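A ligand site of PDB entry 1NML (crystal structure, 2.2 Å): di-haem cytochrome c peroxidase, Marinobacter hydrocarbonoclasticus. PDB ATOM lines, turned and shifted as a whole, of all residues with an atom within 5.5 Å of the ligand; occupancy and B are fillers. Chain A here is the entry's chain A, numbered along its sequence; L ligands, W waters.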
ATOM      1  N   PHE A  38     -26.799  26.737   6.964  1.00  0.00           N
ATOM      2  CA  PHE A  38     -26.564  25.545   6.163  1.00  0.00           C
ATOM      3  C   PHE A  38     -27.257  24.326   6.837  1.00  0.00           C
ATOM      4  O   PHE A  38     -27.783  23.450   6.156  1.00  0.00           O
ATOM      5  CB  PHE A  38     -25.061  25.282   6.021  1.00  0.00           C
ATOM      6  CG  PHE A  38     -24.718  24.173   5.062  1.00  0.00           C
ATOM      7  CD1 PHE A  38     -24.535  24.445   3.702  1.00  0.00           C
ATOM      8  CD2 PHE A  38     -24.573  22.864   5.509  1.00  0.00           C
ATOM      9  CE1 PHE A  38     -24.203  23.420   2.816  1.00  0.00           C
ATOM     10  CE2 PHE A  38     -24.242  21.833   4.630  1.00  0.00           C
ATOM     11  CZ  PHE A  38     -24.057  22.114   3.280  1.00  0.00           C
ATOM     12  N   ILE A  49     -36.169  19.770   6.118  1.00  0.00           N
ATOM     13  CA  ILE A  49     -35.023  19.802   5.211  1.00  0.00           C
ATOM     14  C   ILE A  49     -34.071  20.999   5.365  1.00  0.00           C
ATOM     15  O   ILE A  49     -34.518  22.136   5.513  1.00  0.00           O
ATOM     16  CB  ILE A  49     -35.535  19.757   3.766  1.00  0.00           C
ATOM     17  CG1 ILE A  49     -36.309  18.467   3.529  1.00  0.00           C
ATOM     18  CG2 ILE A  49     -34.398  19.893   2.787  1.00  0.00           C
ATOM     19  CD1 ILE A  49     -37.049  18.437   2.181  1.00  0.00           C
ATOM     20  N   SER A  50     -32.773  20.733   5.309  1.00  0.00           N
ATOM     21  CA  SER A  50     -31.759  21.792   5.378  1.00  0.00           C
ATOM     22  C   SER A  50     -30.767  21.507   4.240  1.00  0.00           C
ATOM     23  O   SER A  50     -30.893  20.485   3.564  1.00  0.00           O
ATOM     24  CB  SER A  50     -31.010  21.748   6.716  1.00  0.00           C
ATOM     25  OG  SER A  50     -30.098  20.659   6.736  1.00  0.00           O
ATOM     26  N   CYS A  51     -29.793  22.388   4.028  1.00  0.00           N
ATOM     27  CA  CYS A  51     -28.811  22.167   2.973  1.00  0.00           C
ATOM     28  C   CYS A  51     -28.079  20.840   3.228  1.00  0.00           C
ATOM     29  O   CYS A  51     -27.840  20.059   2.309  1.00  0.00           O
ATOM     30  CB  CYS A  51     -27.733  23.274   2.964  1.00  0.00           C
ATOM     31  SG  CYS A  51     -28.344  24.985   2.952  1.00  0.00           S
ATOM     32  N   THR A  53     -29.086  18.212   4.478  1.00  0.00           N
ATOM     33  CA  THR A  53     -29.904  17.061   4.123  1.00  0.00           C
ATOM     34  C   THR A  53     -29.471  16.529   2.748  1.00  0.00           C
ATOM     35  O   THR A  53     -29.348  15.315   2.561  1.00  0.00           O
ATOM     36  CB  THR A  53     -31.376  17.448   4.027  1.00  0.00           C
ATOM     37  OG1 THR A  53     -31.814  17.945   5.285  1.00  0.00           O
ATOM     38  CG2 THR A  53     -32.227  16.236   3.622  1.00  0.00           C
ATOM     39  N   CYS A  54     -29.223  17.420   1.792  1.00  0.00           N
ATOM     40  CA  CYS A  54     -28.831  16.972   0.457  1.00  0.00           C
ATOM     41  C   CYS A  54     -27.353  17.101   0.132  1.00  0.00           C
ATOM     42  O   CYS A  54     -26.888  16.579  -0.882  1.00  0.00           O
ATOM     43  CB  CYS A  54     -29.645  17.704  -0.610  1.00  0.00           C
ATOM     44  SG  CYS A  54     -31.455  17.478  -0.466  1.00  0.00           S
ATOM     45  N   HIS A  55     -26.617  17.825   0.985  1.00  0.00           N
ATOM     46  CA  HIS A  55     -25.177  18.019   0.791  1.00  0.00           C
ATOM     47  C   HIS A  55     -24.520  17.702   2.145  1.00  0.00           C
ATOM     48  O   HIS A  55     -23.935  18.553   2.803  1.00  0.00           O
ATOM     49  CB  HIS A  55     -24.881  19.481   0.383  1.00  0.00           C
ATOM     50  CG  HIS A  55     -25.565  19.901  -0.883  1.00  0.00           C
ATOM     51  ND1 HIS A  55     -25.159  19.473  -2.128  1.00  0.00           N
ATOM     52  CD2 HIS A  55     -26.622  20.727  -1.097  1.00  0.00           C
ATOM     53  CE1 HIS A  55     -25.927  20.018  -3.052  1.00  0.00           C
ATOM     54  NE2 HIS A  55     -26.823  20.786  -2.454  1.00  0.00           N
ATOM     55  N   ASP A  63     -25.856  13.995  -2.009  1.00  0.00           N
ATOM     56  CA  ASP A  63     -26.985  13.148  -1.609  1.00  0.00           C
ATOM     57  C   ASP A  63     -26.849  11.776  -2.227  1.00  0.00           C
ATOM     58  O   ASP A  63     -26.372  11.617  -3.345  1.00  0.00           O
ATOM     59  CB  ASP A  63     -28.281  13.798  -2.096  1.00  0.00           C
ATOM     60  CG  ASP A  63     -29.525  13.224  -1.433  1.00  0.00           C
ATOM     61  OD1 ASP A  63     -30.622  13.781  -1.682  1.00  0.00           O
ATOM     62  OD2 ASP A  63     -29.421  12.245  -0.680  1.00  0.00           O
ATOM     63  N   THR A  67     -33.065  13.376  -6.493  1.00  0.00           N
ATOM     64  CA  THR A  67     -34.207  14.077  -5.906  1.00  0.00           C
ATOM     65  C   THR A  67     -34.852  15.035  -6.904  1.00  0.00           C
ATOM     66  O   THR A  67     -34.215  15.480  -7.859  1.00  0.00           O
ATOM     67  CB  THR A  67     -33.773  14.850  -4.639  1.00  0.00           C
ATOM     68  OG1 THR A  67     -34.886  15.610  -4.142  1.00  0.00           O
ATOM     69  CG2 THR A  67     -32.636  15.796  -4.947  1.00  0.00           C
ATOM     70  N   ILE A  69     -36.659  17.755  -5.605  1.00  0.00           N
ATOM     71  CA  ILE A  69     -36.853  19.019  -4.922  1.00  0.00           C
ATOM     72  C   ILE A  69     -35.562  19.768  -4.614  1.00  0.00           C
ATOM     73  O   ILE A  69     -34.469  19.288  -4.915  1.00  0.00           O
ATOM     74  CB  ILE A  69     -37.657  18.818  -3.618  1.00  0.00           C
ATOM     75  CG1 ILE A  69     -36.966  17.796  -2.723  1.00  0.00           C
ATOM     76  CG2 ILE A  69     -39.070  18.314  -3.951  1.00  0.00           C
ATOM     77  CD1 ILE A  69     -37.508  17.785  -1.321  1.00  0.00           C
ATOM     78  N   GLY A  70     -35.707  20.955  -4.031  1.00  0.00           N
ATOM     79  CA  GLY A  70     -34.568  21.790  -3.723  1.00  0.00           C
ATOM     80  C   GLY A  70     -34.350  22.792  -4.846  1.00  0.00           C
ATOM     81  O   GLY A  70     -34.585  22.481  -6.013  1.00  0.00           O
ATOM     82  N   HIS A  71     -33.918  24.005  -4.486  1.00  0.00           N
ATOM     83  CA  HIS A  71     -33.648  25.078  -5.449  1.00  0.00           C
ATOM     84  C   HIS A  71     -34.811  25.395  -6.402  1.00  0.00           C
ATOM     85  O   HIS A  71     -34.603  25.690  -7.568  1.00  0.00           O
ATOM     86  CB  HIS A  71     -32.398  24.718  -6.250  1.00  0.00           C
ATOM     87  CG  HIS A  71     -31.209  24.444  -5.389  1.00  0.00           C
ATOM     88  ND1 HIS A  71     -30.649  25.405  -4.568  1.00  0.00           N
ATOM     89  CD2 HIS A  71     -30.504  23.311  -5.169  1.00  0.00           C
ATOM     90  CE1 HIS A  71     -29.649  24.866  -3.886  1.00  0.00           C
ATOM     91  NE2 HIS A  71     -29.553  23.596  -4.226  1.00  0.00           N
ATOM     92  N   TRP A  73     -36.704  23.618  -7.945  1.00  0.00           N
ATOM     93  CA  TRP A  73     -36.727  22.735  -9.103  1.00  0.00           C
ATOM     94  C   TRP A  73     -38.150  22.217  -9.326  1.00  0.00           C
ATOM     95  O   TRP A  73     -38.833  21.840  -8.376  1.00  0.00           O
ATOM     96  CB  TRP A  73     -35.775  21.567  -8.870  1.00  0.00           C
ATOM     97  CG  TRP A  73     -35.608  20.623 -10.024  1.00  0.00           C
ATOM     98  CD1 TRP A  73     -36.424  19.582 -10.347  1.00  0.00           C
ATOM     99  CD2 TRP A  73     -34.514  20.580 -10.944  1.00  0.00           C
ATOM    100  NE1 TRP A  73     -35.908  18.881 -11.401  1.00  0.00           N
ATOM    101  CE2 TRP A  73     -34.727  19.469 -11.792  1.00  0.00           C
ATOM    102  CE3 TRP A  73     -33.364  21.358 -11.126  1.00  0.00           C
ATOM    103  CZ2 TRP A  73     -33.831  19.124 -12.828  1.00  0.00           C
ATOM    104  CZ3 TRP A  73     -32.460  21.009 -12.151  1.00  0.00           C
ATOM    105  CH2 TRP A  73     -32.717  19.903 -12.991  1.00  0.00           C
ATOM    106  N   ARG A  78     -32.956  14.482 -10.219  1.00  0.00           N
ATOM    107  CA  ARG A  78     -31.605  14.590 -10.731  1.00  0.00           C
ATOM    108  C   ARG A  78     -30.650  14.327  -9.573  1.00  0.00           C
ATOM    109  O   ARG A  78     -31.032  14.378  -8.407  1.00  0.00           O
ATOM    110  CB  ARG A  78     -31.361  15.985 -11.323  1.00  0.00           C
ATOM    111  CG  ARG A  78     -30.997  17.073 -10.323  1.00  0.00           C
ATOM    112  CD  ARG A  78     -32.034  18.179 -10.220  1.00  0.00           C
ATOM    113  NE  ARG A  78     -32.944  17.954  -9.116  1.00  0.00           N
ATOM    114  CZ  ARG A  78     -33.286  18.862  -8.202  1.00  0.00           C
ATOM    115  NH1 ARG A  78     -32.792  20.091  -8.239  1.00  0.00           N
ATOM    116  NH2 ARG A  78     -34.106  18.521  -7.224  1.00  0.00           N
ATOM    117  N   ASN A  79     -29.399  14.017  -9.901  1.00  0.00           N
ATOM    118  CA  ASN A  79     -28.371  13.739  -8.904  1.00  0.00           C
ATOM    119  C   ASN A  79     -27.938  15.069  -8.284  1.00  0.00           C
ATOM    120  O   ASN A  79     -28.158  16.122  -8.860  1.00  0.00           O
ATOM    121  CB  ASN A  79     -27.184  13.070  -9.589  1.00  0.00           C
ATOM    122  CG  ASN A  79     -26.207  12.457  -8.609  1.00  0.00           C
ATOM    123  OD1 ASN A  79     -25.076  12.115  -8.980  1.00  0.00           O
ATOM    124  ND2 ASN A  79     -26.622  12.305  -7.360  1.00  0.00           N
ATOM    125  N   SER A  80     -27.327  15.016  -7.099  1.00  0.00           N
ATOM    126  CA  SER A  80     -26.877  16.249  -6.468  1.00  0.00           C
ATOM    127  C   SER A  80     -25.351  16.294  -6.488  1.00  0.00           C
ATOM    128  O   SER A  80     -24.680  15.296  -6.208  1.00  0.00           O
ATOM    129  CB  SER A  80     -27.362  16.332  -5.035  1.00  0.00           C
ATOM    130  OG  SER A  80     -26.731  15.343  -4.248  1.00  0.00           O
ATOM    131  N   PRO A  81     -24.785  17.459  -6.841  1.00  0.00           N
ATOM    132  CA  PRO A  81     -23.347  17.661  -6.890  1.00  0.00           C
ATOM    133  C   PRO A  81     -22.864  17.868  -5.456  1.00  0.00           C
ATOM    134  O   PRO A  81     -23.679  18.120  -4.566  1.00  0.00           O
ATOM    135  CB  PRO A  81     -23.199  18.915  -7.730  1.00  0.00           C
ATOM    136  CG  PRO A  81     -24.396  19.718  -7.282  1.00  0.00           C
ATOM    137  CD  PRO A  81     -25.496  18.686  -7.238  1.00  0.00           C
ATOM    138  N   THR A  82     -21.556  17.770  -5.232  1.00  0.00           N
ATOM    139  CA  THR A  82     -21.006  17.961  -3.906  1.00  0.00           C
ATOM    140  C   THR A  82     -20.756  19.451  -3.680  1.00  0.00           C
ATOM    141  O   THR A  82     -20.424  20.171  -4.634  1.00  0.00           O
ATOM    142  CB  THR A  82     -19.658  17.235  -3.738  1.00  0.00           C
ATOM    143  OG1 THR A  82     -19.097  17.569  -2.457  1.00  0.00           O
ATOM    144  CG2 THR A  82     -18.664  17.654  -4.837  1.00  0.00           C
ATOM    145  N   VAL A  83     -20.904  19.910  -2.442  1.00  0.00           N
ATOM    146  CA  VAL A  83     -20.608  21.298  -2.147  1.00  0.00           C
ATOM    147  C   VAL A  83     -19.096  21.459  -1.980  1.00  0.00           C
ATOM    148  O   VAL A  83     -18.577  22.571  -2.050  1.00  0.00           O
ATOM    149  CB  VAL A  83     -21.307  21.804  -0.860  1.00  0.00           C
ATOM    150  CG1 VAL A  83     -22.805  21.929  -1.105  1.00  0.00           C
ATOM    151  CG2 VAL A  83     -21.038  20.856   0.306  1.00  0.00           C
ATOM    152  N   ALA A  86     -16.907  23.446  -4.538  1.00  0.00           N
ATOM    153  CA  ALA A  86     -17.812  23.977  -5.550  1.00  0.00           C
ATOM    154  C   ALA A  86     -17.419  25.415  -5.901  1.00  0.00           C
ATOM    155  O   ALA A  86     -17.587  25.862  -7.033  1.00  0.00           O
ATOM    156  CB  ALA A  86     -19.251  23.925  -5.047  1.00  0.00           C
ATOM    157  N   ASN A  89     -15.508  26.079  -9.144  1.00  0.00           N
ATOM    158  CA  ASN A  89     -16.100  25.792 -10.443  1.00  0.00           C
ATOM    159  C   ASN A  89     -16.735  27.041 -11.050  1.00  0.00           C
ATOM    160  O   ASN A  89     -17.487  27.739 -10.384  1.00  0.00           O
ATOM    161  CB  ASN A  89     -17.167  24.688 -10.347  1.00  0.00           C
ATOM    162  CG  ASN A  89     -16.631  23.377  -9.781  1.00  0.00           C
ATOM    163  OD1 ASN A  89     -15.591  22.876 -10.210  1.00  0.00           O
ATOM    164  ND2 ASN A  89     -17.360  22.788  -8.828  1.00  0.00           N
ATOM    165  N   ALA A  91     -18.529  26.820 -13.899  1.00  0.00           N
ATOM    166  CA  ALA A  91     -19.817  26.328 -14.397  1.00  0.00           C
ATOM    167  C   ALA A  91     -20.533  25.668 -13.231  1.00  0.00           C
ATOM    168  O   ALA A  91     -19.899  25.248 -12.280  1.00  0.00           O
ATOM    169  CB  ALA A  91     -19.609  25.326 -15.525  1.00  0.00           C
ATOM    170  N   GLN A  92     -21.855  25.572 -13.306  1.00  0.00           N
ATOM    171  CA  GLN A  92     -22.629  24.921 -12.256  1.00  0.00           C
ATOM    172  C   GLN A  92     -23.214  23.623 -12.800  1.00  0.00           C
ATOM    173  O   GLN A  92     -23.257  23.398 -14.021  1.00  0.00           O
ATOM    174  CB  GLN A  92     -23.768  25.826 -11.784  1.00  0.00           C
ATOM    175  CG  GLN A  92     -24.835  26.127 -12.852  1.00  0.00           C
ATOM    176  CD  GLN A  92     -26.218  26.423 -12.266  1.00  0.00           C
ATOM    177  OE1 GLN A  92     -26.918  25.526 -11.781  1.00  0.00           O
ATOM    178  NE2 GLN A  92     -26.601  27.692 -12.270  1.00  0.00           N
ATOM    179  N   PHE A  93     -23.658  22.770 -11.884  1.00  0.00           N
ATOM    180  CA  PHE A  93     -24.294  21.509 -12.254  1.00  0.00           C
ATOM    181  C   PHE A  93     -25.386  21.874 -13.256  1.00  0.00           C
ATOM    182  O   PHE A  93     -26.143  22.822 -13.038  1.00  0.00           O
ATOM    183  CB  PHE A  93     -24.955  20.883 -11.017  1.00  0.00           C
ATOM    184  CG  PHE A  93     -25.846  19.705 -11.332  1.00  0.00           C
ATOM    185  CD1 PHE A  93     -25.422  18.406 -11.042  1.00  0.00           C
ATOM    186  CD2 PHE A  93     -27.121  19.883 -11.874  1.00  0.00           C
ATOM    187  CE1 PHE A  93     -26.245  17.308 -11.295  1.00  0.00           C
ATOM    188  CE2 PHE A  93     -27.958  18.789 -12.126  1.00  0.00           C
ATOM    189  CZ  PHE A  93     -27.517  17.496 -11.827  1.00  0.00           C
ATOM    190  N   PRO A 108     -21.785  28.199  -8.998  1.00  0.00           N
ATOM    191  CA  PRO A 108     -22.230  27.183  -8.039  1.00  0.00           C
ATOM    192  C   PRO A 108     -22.685  27.796  -6.720  1.00  0.00           C
ATOM    193  O   PRO A 108     -23.761  27.494  -6.208  1.00  0.00           O
ATOM    194  CB  PRO A 108     -20.977  26.326  -7.834  1.00  0.00           C
ATOM    195  CG  PRO A 108     -20.232  26.476  -9.129  1.00  0.00           C
ATOM    196  CD  PRO A 108     -20.402  27.948  -9.446  1.00  0.00           C
ATOM    197  N   VAL A 109     -21.828  28.657  -6.166  1.00  0.00           N
ATOM    198  CA  VAL A 109     -22.096  29.310  -4.903  1.00  0.00           C
ATOM    199  C   VAL A 109     -23.423  30.052  -4.928  1.00  0.00           C
ATOM    200  O   VAL A 109     -24.207  29.969  -3.966  1.00  0.00           O
ATOM    201  CB  VAL A 109     -20.919  30.247  -4.534  1.00  0.00           C
ATOM    202  CG1 VAL A 109     -21.331  31.237  -3.465  1.00  0.00           C
ATOM    203  CG2 VAL A 109     -19.747  29.396  -4.041  1.00  0.00           C
ATOM    204  N   ALA A 111     -25.875  29.522  -7.254  1.00  0.00           N
ATOM    205  CA  ALA A 111     -26.938  28.567  -7.557  1.00  0.00           C
ATOM    206  C   ALA A 111     -27.384  27.889  -6.261  1.00  0.00           C
ATOM    207  O   ALA A 111     -28.555  27.532  -6.097  1.00  0.00           O
ATOM    208  CB  ALA A 111     -26.434  27.533  -8.548  1.00  0.00           C
ATOM    209  N   GLY A 112     -26.433  27.730  -5.352  1.00  0.00           N
ATOM    210  CA  GLY A 112     -26.726  27.104  -4.082  1.00  0.00           C
ATOM    211  C   GLY A 112     -27.754  27.828  -3.225  1.00  0.00           C
ATOM    212  O   GLY A 112     -28.424  27.195  -2.409  1.00  0.00           O
ATOM    213  N   VAL A 113     -27.870  29.141  -3.386  1.00  0.00           N
ATOM    214  CA  VAL A 113     -28.836  29.880  -2.583  1.00  0.00           C
ATOM    215  C   VAL A 113     -30.155  30.148  -3.274  1.00  0.00           C
ATOM    216  O   VAL A 113     -30.957  30.947  -2.818  1.00  0.00           O
ATOM    217  CB  VAL A 113     -28.242  31.212  -2.034  1.00  0.00           C
ATOM    218  CG1 VAL A 113     -27.149  30.878  -1.032  1.00  0.00           C
ATOM    219  CG2 VAL A 113     -27.688  32.079  -3.173  1.00  0.00           C
ATOM    220  N   GLU A 114     -30.378  29.463  -4.395  1.00  0.00           N
ATOM    221  CA  GLU A 114     -31.661  29.550  -5.078  1.00  0.00           C
ATOM    222  C   GLU A 114     -32.534  28.687  -4.164  1.00  0.00           C
ATOM    223  O   GLU A 114     -32.186  27.538  -3.879  1.00  0.00           O
ATOM    224  CB  GLU A 114     -31.579  28.921  -6.474  1.00  0.00           C
ATOM    225  CG  GLU A 114     -30.842  29.780  -7.507  1.00  0.00           C
ATOM    226  CD  GLU A 114     -30.456  29.022  -8.783  1.00  0.00           C
ATOM    227  OE1 GLU A 114     -31.024  27.945  -9.052  1.00  0.00           O
ATOM    228  OE2 GLU A 114     -29.575  29.510  -9.515  1.00  0.00           O
ATOM    229  N   MET A 115     -33.660  29.224  -3.694  1.00  0.00           N
ATOM    230  CA  MET A 115     -34.518  28.467  -2.789  1.00  0.00           C
ATOM    231  C   MET A 115     -35.943  28.218  -3.263  1.00  0.00           C
ATOM    232  O   MET A 115     -36.472  28.927  -4.118  1.00  0.00           O
ATOM    233  CB  MET A 115     -34.566  29.165  -1.432  1.00  0.00           C
ATOM    234  CG  MET A 115     -33.219  29.253  -0.740  1.00  0.00           C
ATOM    235  SD  MET A 115     -33.387  29.789   0.950  1.00  0.00           S
ATOM    236  CE  MET A 115     -31.791  29.308   1.608  1.00  0.00           C
ATOM    237  N   ILE A 156     -24.642  32.475   3.675  1.00  0.00           N
ATOM    238  CA  ILE A 156     -24.551  31.086   3.252  1.00  0.00           C
ATOM    239  C   ILE A 156     -23.398  30.918   2.245  1.00  0.00           C
ATOM    240  O   ILE A 156     -22.604  29.980   2.334  1.00  0.00           O
ATOM    241  CB  ILE A 156     -25.883  30.607   2.631  1.00  0.00           C
ATOM    242  CG1 ILE A 156     -26.968  30.569   3.713  1.00  0.00           C
ATOM    243  CG2 ILE A 156     -25.696  29.233   2.010  1.00  0.00           C
ATOM    244  CD1 ILE A 156     -28.349  30.218   3.184  1.00  0.00           C
ATOM    245  N   GLU A 160     -20.279  28.468   2.196  1.00  0.00           N
ATOM    246  CA  GLU A 160     -20.019  27.567   1.063  1.00  0.00           C
ATOM    247  C   GLU A 160     -18.568  27.688   0.599  1.00  0.00           C
ATOM    248  O   GLU A 160     -17.939  26.689   0.234  1.00  0.00           O
ATOM    249  CB  GLU A 160     -20.920  27.892  -0.123  1.00  0.00           C
ATOM    250  CG  GLU A 160     -22.378  27.507   0.056  1.00  0.00           C
ATOM    251  CD  GLU A 160     -23.217  27.899  -1.135  1.00  0.00           C
ATOM    252  OE1 GLU A 160     -23.699  26.998  -1.856  1.00  0.00           O
ATOM    253  OE2 GLU A 160     -23.399  29.115  -1.374  1.00  0.00           O
ATOM    254  N   ARG A 246     -22.518  19.697 -17.397  1.00  0.00           N
ATOM    255  CA  ARG A 246     -21.246  20.243 -16.991  1.00  0.00           C
ATOM    256  C   ARG A 246     -20.259  19.071 -16.836  1.00  0.00           C
ATOM    257  O   ARG A 246     -20.629  18.014 -16.323  1.00  0.00           O
ATOM    258  CB  ARG A 246     -21.417  20.949 -15.656  1.00  0.00           C
ATOM    259  CG  ARG A 246     -20.145  21.424 -15.013  1.00  0.00           C
ATOM    260  CD  ARG A 246     -20.216  20.948 -13.593  1.00  0.00           C
ATOM    261  NE  ARG A 246     -20.032  22.026 -12.672  1.00  0.00           N
ATOM    262  CZ  ARG A 246     -20.225  21.929 -11.362  1.00  0.00           C
ATOM    263  NH1 ARG A 246     -20.613  20.783 -10.825  1.00  0.00           N
ATOM    264  NH2 ARG A 246     -19.983  22.993 -10.620  1.00  0.00           N
HETATM  265 FE1  LIG L   1     -28.134  22.156  -3.304  1.00  0.00          FE
HETATM  266  C1  LIG L   1     -26.791  22.046  -6.332  1.00  0.00           C
HETATM  267  C2  LIG L   1     -25.729  24.349  -2.248  1.00  0.00           C
HETATM  268  C3  LIG L   1     -29.961  22.893  -0.589  1.00  0.00           C
HETATM  269  C4  LIG L   1     -30.156  19.582  -4.011  1.00  0.00           C
HETATM  270  N1  LIG L   1     -26.510  23.016  -4.137  1.00  0.00           N
HETATM  271  C5  LIG L   1     -26.116  22.835  -5.434  1.00  0.00           C
HETATM  272  C6  LIG L   1     -24.865  23.579  -5.623  1.00  0.00           C
HETATM  273  C7  LIG L   1     -24.506  24.119  -4.437  1.00  0.00           C
HETATM  274  C8  LIG L   1     -25.600  23.851  -3.512  1.00  0.00           C
HETATM  275  C9  LIG L   1     -23.237  24.916  -4.078  1.00  0.00           C
HETATM  276  C10 LIG L   1     -24.094  23.618  -6.958  1.00  0.00           C
HETATM  277  C11 LIG L   1     -22.764  22.863  -6.972  1.00  0.00           C
HETATM  278  C12 LIG L   1     -22.021  22.956  -8.292  1.00  0.00           C
HETATM  279  O1  LIG L   1     -20.782  22.682  -8.218  1.00  0.00           O
HETATM  280  O2  LIG L   1     -22.620  23.222  -9.335  1.00  0.00           O
HETATM  281  N2  LIG L   1     -27.903  23.412  -1.755  1.00  0.00           N
HETATM  282  C13 LIG L   1     -26.834  24.233  -1.462  1.00  0.00           C
HETATM  283  C14 LIG L   1     -27.029  24.994  -0.248  1.00  0.00           C
HETATM  284  C15 LIG L   1     -28.285  24.656   0.159  1.00  0.00           C
HETATM  285  C16 LIG L   1     -28.782  23.636  -0.714  1.00  0.00           C
HETATM  286  C17 LIG L   1     -26.018  26.006   0.342  1.00  0.00           C
HETATM  287  C18 LIG L   1     -29.114  25.177   1.347  1.00  0.00           C
HETATM  288  C19 LIG L   1     -29.510  26.671   1.160  1.00  0.00           C
HETATM  289  N3  LIG L   1     -29.757  21.352  -2.447  1.00  0.00           N
HETATM  290  C20 LIG L   1     -30.362  21.785  -1.301  1.00  0.00           C
HETATM  291  C21 LIG L   1     -31.402  20.835  -0.905  1.00  0.00           C
HETATM  292  C22 LIG L   1     -31.417  19.860  -1.829  1.00  0.00           C
HETATM  293  C23 LIG L   1     -30.395  20.187  -2.812  1.00  0.00           C
HETATM  294  C24 LIG L   1     -32.229  20.992   0.403  1.00  0.00           C
HETATM  295  C25 LIG L   1     -32.239  18.544  -1.881  1.00  0.00           C
HETATM  296  C26 LIG L   1     -33.773  18.576  -1.835  1.00  0.00           C
HETATM  297  N4  LIG L   1     -28.442  21.049  -4.900  1.00  0.00           N
HETATM  298  C27 LIG L   1     -29.343  19.980  -5.035  1.00  0.00           C
HETATM  299  C28 LIG L   1     -29.293  19.419  -6.376  1.00  0.00           C
HETATM  300  C29 LIG L   1     -28.431  20.201  -7.092  1.00  0.00           C
HETATM  301  C30 LIG L   1     -27.835  21.150  -6.135  1.00  0.00           C
HETATM  302  C31 LIG L   1     -30.129  18.214  -6.896  1.00  0.00           C
HETATM  303  C32 LIG L   1     -28.190  20.015  -8.623  1.00  0.00           C
HETATM  304  C33 LIG L   1     -29.064  21.254  -8.869  1.00  0.00           C
HETATM  305  C34 LIG L   1     -29.812  22.413  -9.391  1.00  0.00           C
HETATM  306  O3  LIG L   1     -28.902  23.247  -9.166  1.00  0.00           O
HETATM  307  O4  LIG L   1     -30.925  22.496  -8.867  1.00  0.00           O
HETATM  308  O   HOH W   1     -29.371  25.774  -8.122  1.00  0.00           O
HETATM  309  O   HOH W   2     -32.680  24.781  -9.963  1.00  0.00           O
HETATM  310  O   HOH W   3     -30.100  25.382 -11.547  1.00  0.00           O
HETATM  311  O   HOH W   4     -29.452  22.792 -12.675  1.00  0.00           O
HETATM  312  O   HOH W   5     -19.626  20.490  -7.208  1.00  0.00           O
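The side-chain sulfur (SG) of Cys 51 is covalently linked to a carbon (C18) of the ligand (1.8 Å).
SG of Cys 54 is bonded to C25 of the ligand, 1.9 Å away.
A ring nitrogen (NE2) of His 55 binds an iron atom (FE1) of the ligand (2.1 Å).
A ring nitrogen (NE2) of His 71 binds an iron atom (FE1) of the ligand (2.2 Å).
An oxygen (O1) of the ligand lies within salt-bridge range of the guanidinium group (NH2) of Arg 246 (2.6 Å).
N of Phe 93 sits at hydrogen-bond distance from O2 of the ligand, 2.8 Å away.
The guanidinium group of Arg 78 lies within salt-bridge range of an oxygen (O4) of the ligand.
An oxygen (O1) of the ligand sits at hydrogen-bond distance from the side-chain amide nitrogen (ND2) of Asn 89 (3.5 Å).
CD1 of Phe 38 touches C17 of the ligand, 3.99 Å away.
Ile 49 touches the ligand.
Ser 50 touches the ligand.
OG1 of Thr 67 touches C26 of the ligand (3.9 Å).
Ile 69 touches the ligand.
N of Gly 70 touches C26 of the ligand, at 3.8 Å.
Trp 73 touches the ligand.
Asn 79 touches the ligand.
Ser 80 touches the ligand.
Pro 81 touches the ligand (CD to C29, 3.3 Å).
Val 83 touches the ligand (CG1 to C2, 3.96 Å).
Ala 86 touches the ligand.
Gln 92 touches the ligand.
Pro 108 touches the ligand (O to C9, 3.4 Å).
Gly 112 touches the ligand (O to C14, 3.4 Å).
CE of Met 115 touches C19 of the ligand, at 3.5 Å.
Ile 156 touches the ligand.
Glu 160 touches the ligand.
Within 4 Å of the ligand: Phe 38, Ile 49, Ser 50, Cys 51, Cys 54, His 55, Thr 67, Ile 69, Gly 70, His 71, Trp 73, Arg 78, Asn 79, Ser 80, Pro 81, Val 83, Ala 86, Asn 89, Gln 92, Phe 93, Pro 108, Gly 112, Met 115, Ile 156, Glu 160 and Arg 246.
Water W5 bridges an oxygen (O1) of the ligand (2.7 Å) and the backbone carbonyl oxygen of Thr 82 (2.7 Å).
Water W1 lies within hydrogen-bond range of an oxygen (O3) of the ligand (2.8 Å), the backbone carbonyl oxygen of Ala 111 (2.8 Å) and the side-chain carboxylate of Glu 114 (2.9 Å).
Water W2 lies within hydrogen-bond range of O4 of the ligand and O of His 71.
Water W3 lies within hydrogen-bond range of OE1 of Gln 92 (3.2 Å) and O3 of the ligand (3.4 Å).
The backbone NH (N) of Asp 63 lies within hydrogen-bond range of the backbone carbonyl oxygen (O) of Cys 54.
A ring nitrogen (ND1) of His 71 is in hydrogen-bond range of the backbone carbonyl oxygen (O) of Ala 111, at 3.4 Å.
NH2 of Arg 246 lies close to ND2 of Asn 89, 3.2 Å away.
NH2 of Arg 246 sits at hydrogen-bond distance from O of Ala 91 (2.8 Å).
NH2 of Arg 78 sits at hydrogen-bond distance from O of Ile 69 (2.5 Å).
N of Arg 78 is in hydrogen-bond range of O of Thr 67 (2.9 Å).
The backbone NH of Ile 69 is in hydrogen-bond range of the side-chain hydroxyl of Thr 67, 3.1 Å away.
The backbone NH (N) of Ser 50 is in hydrogen-bond range of the side-chain hydroxyl (OG1) of Thr 53.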
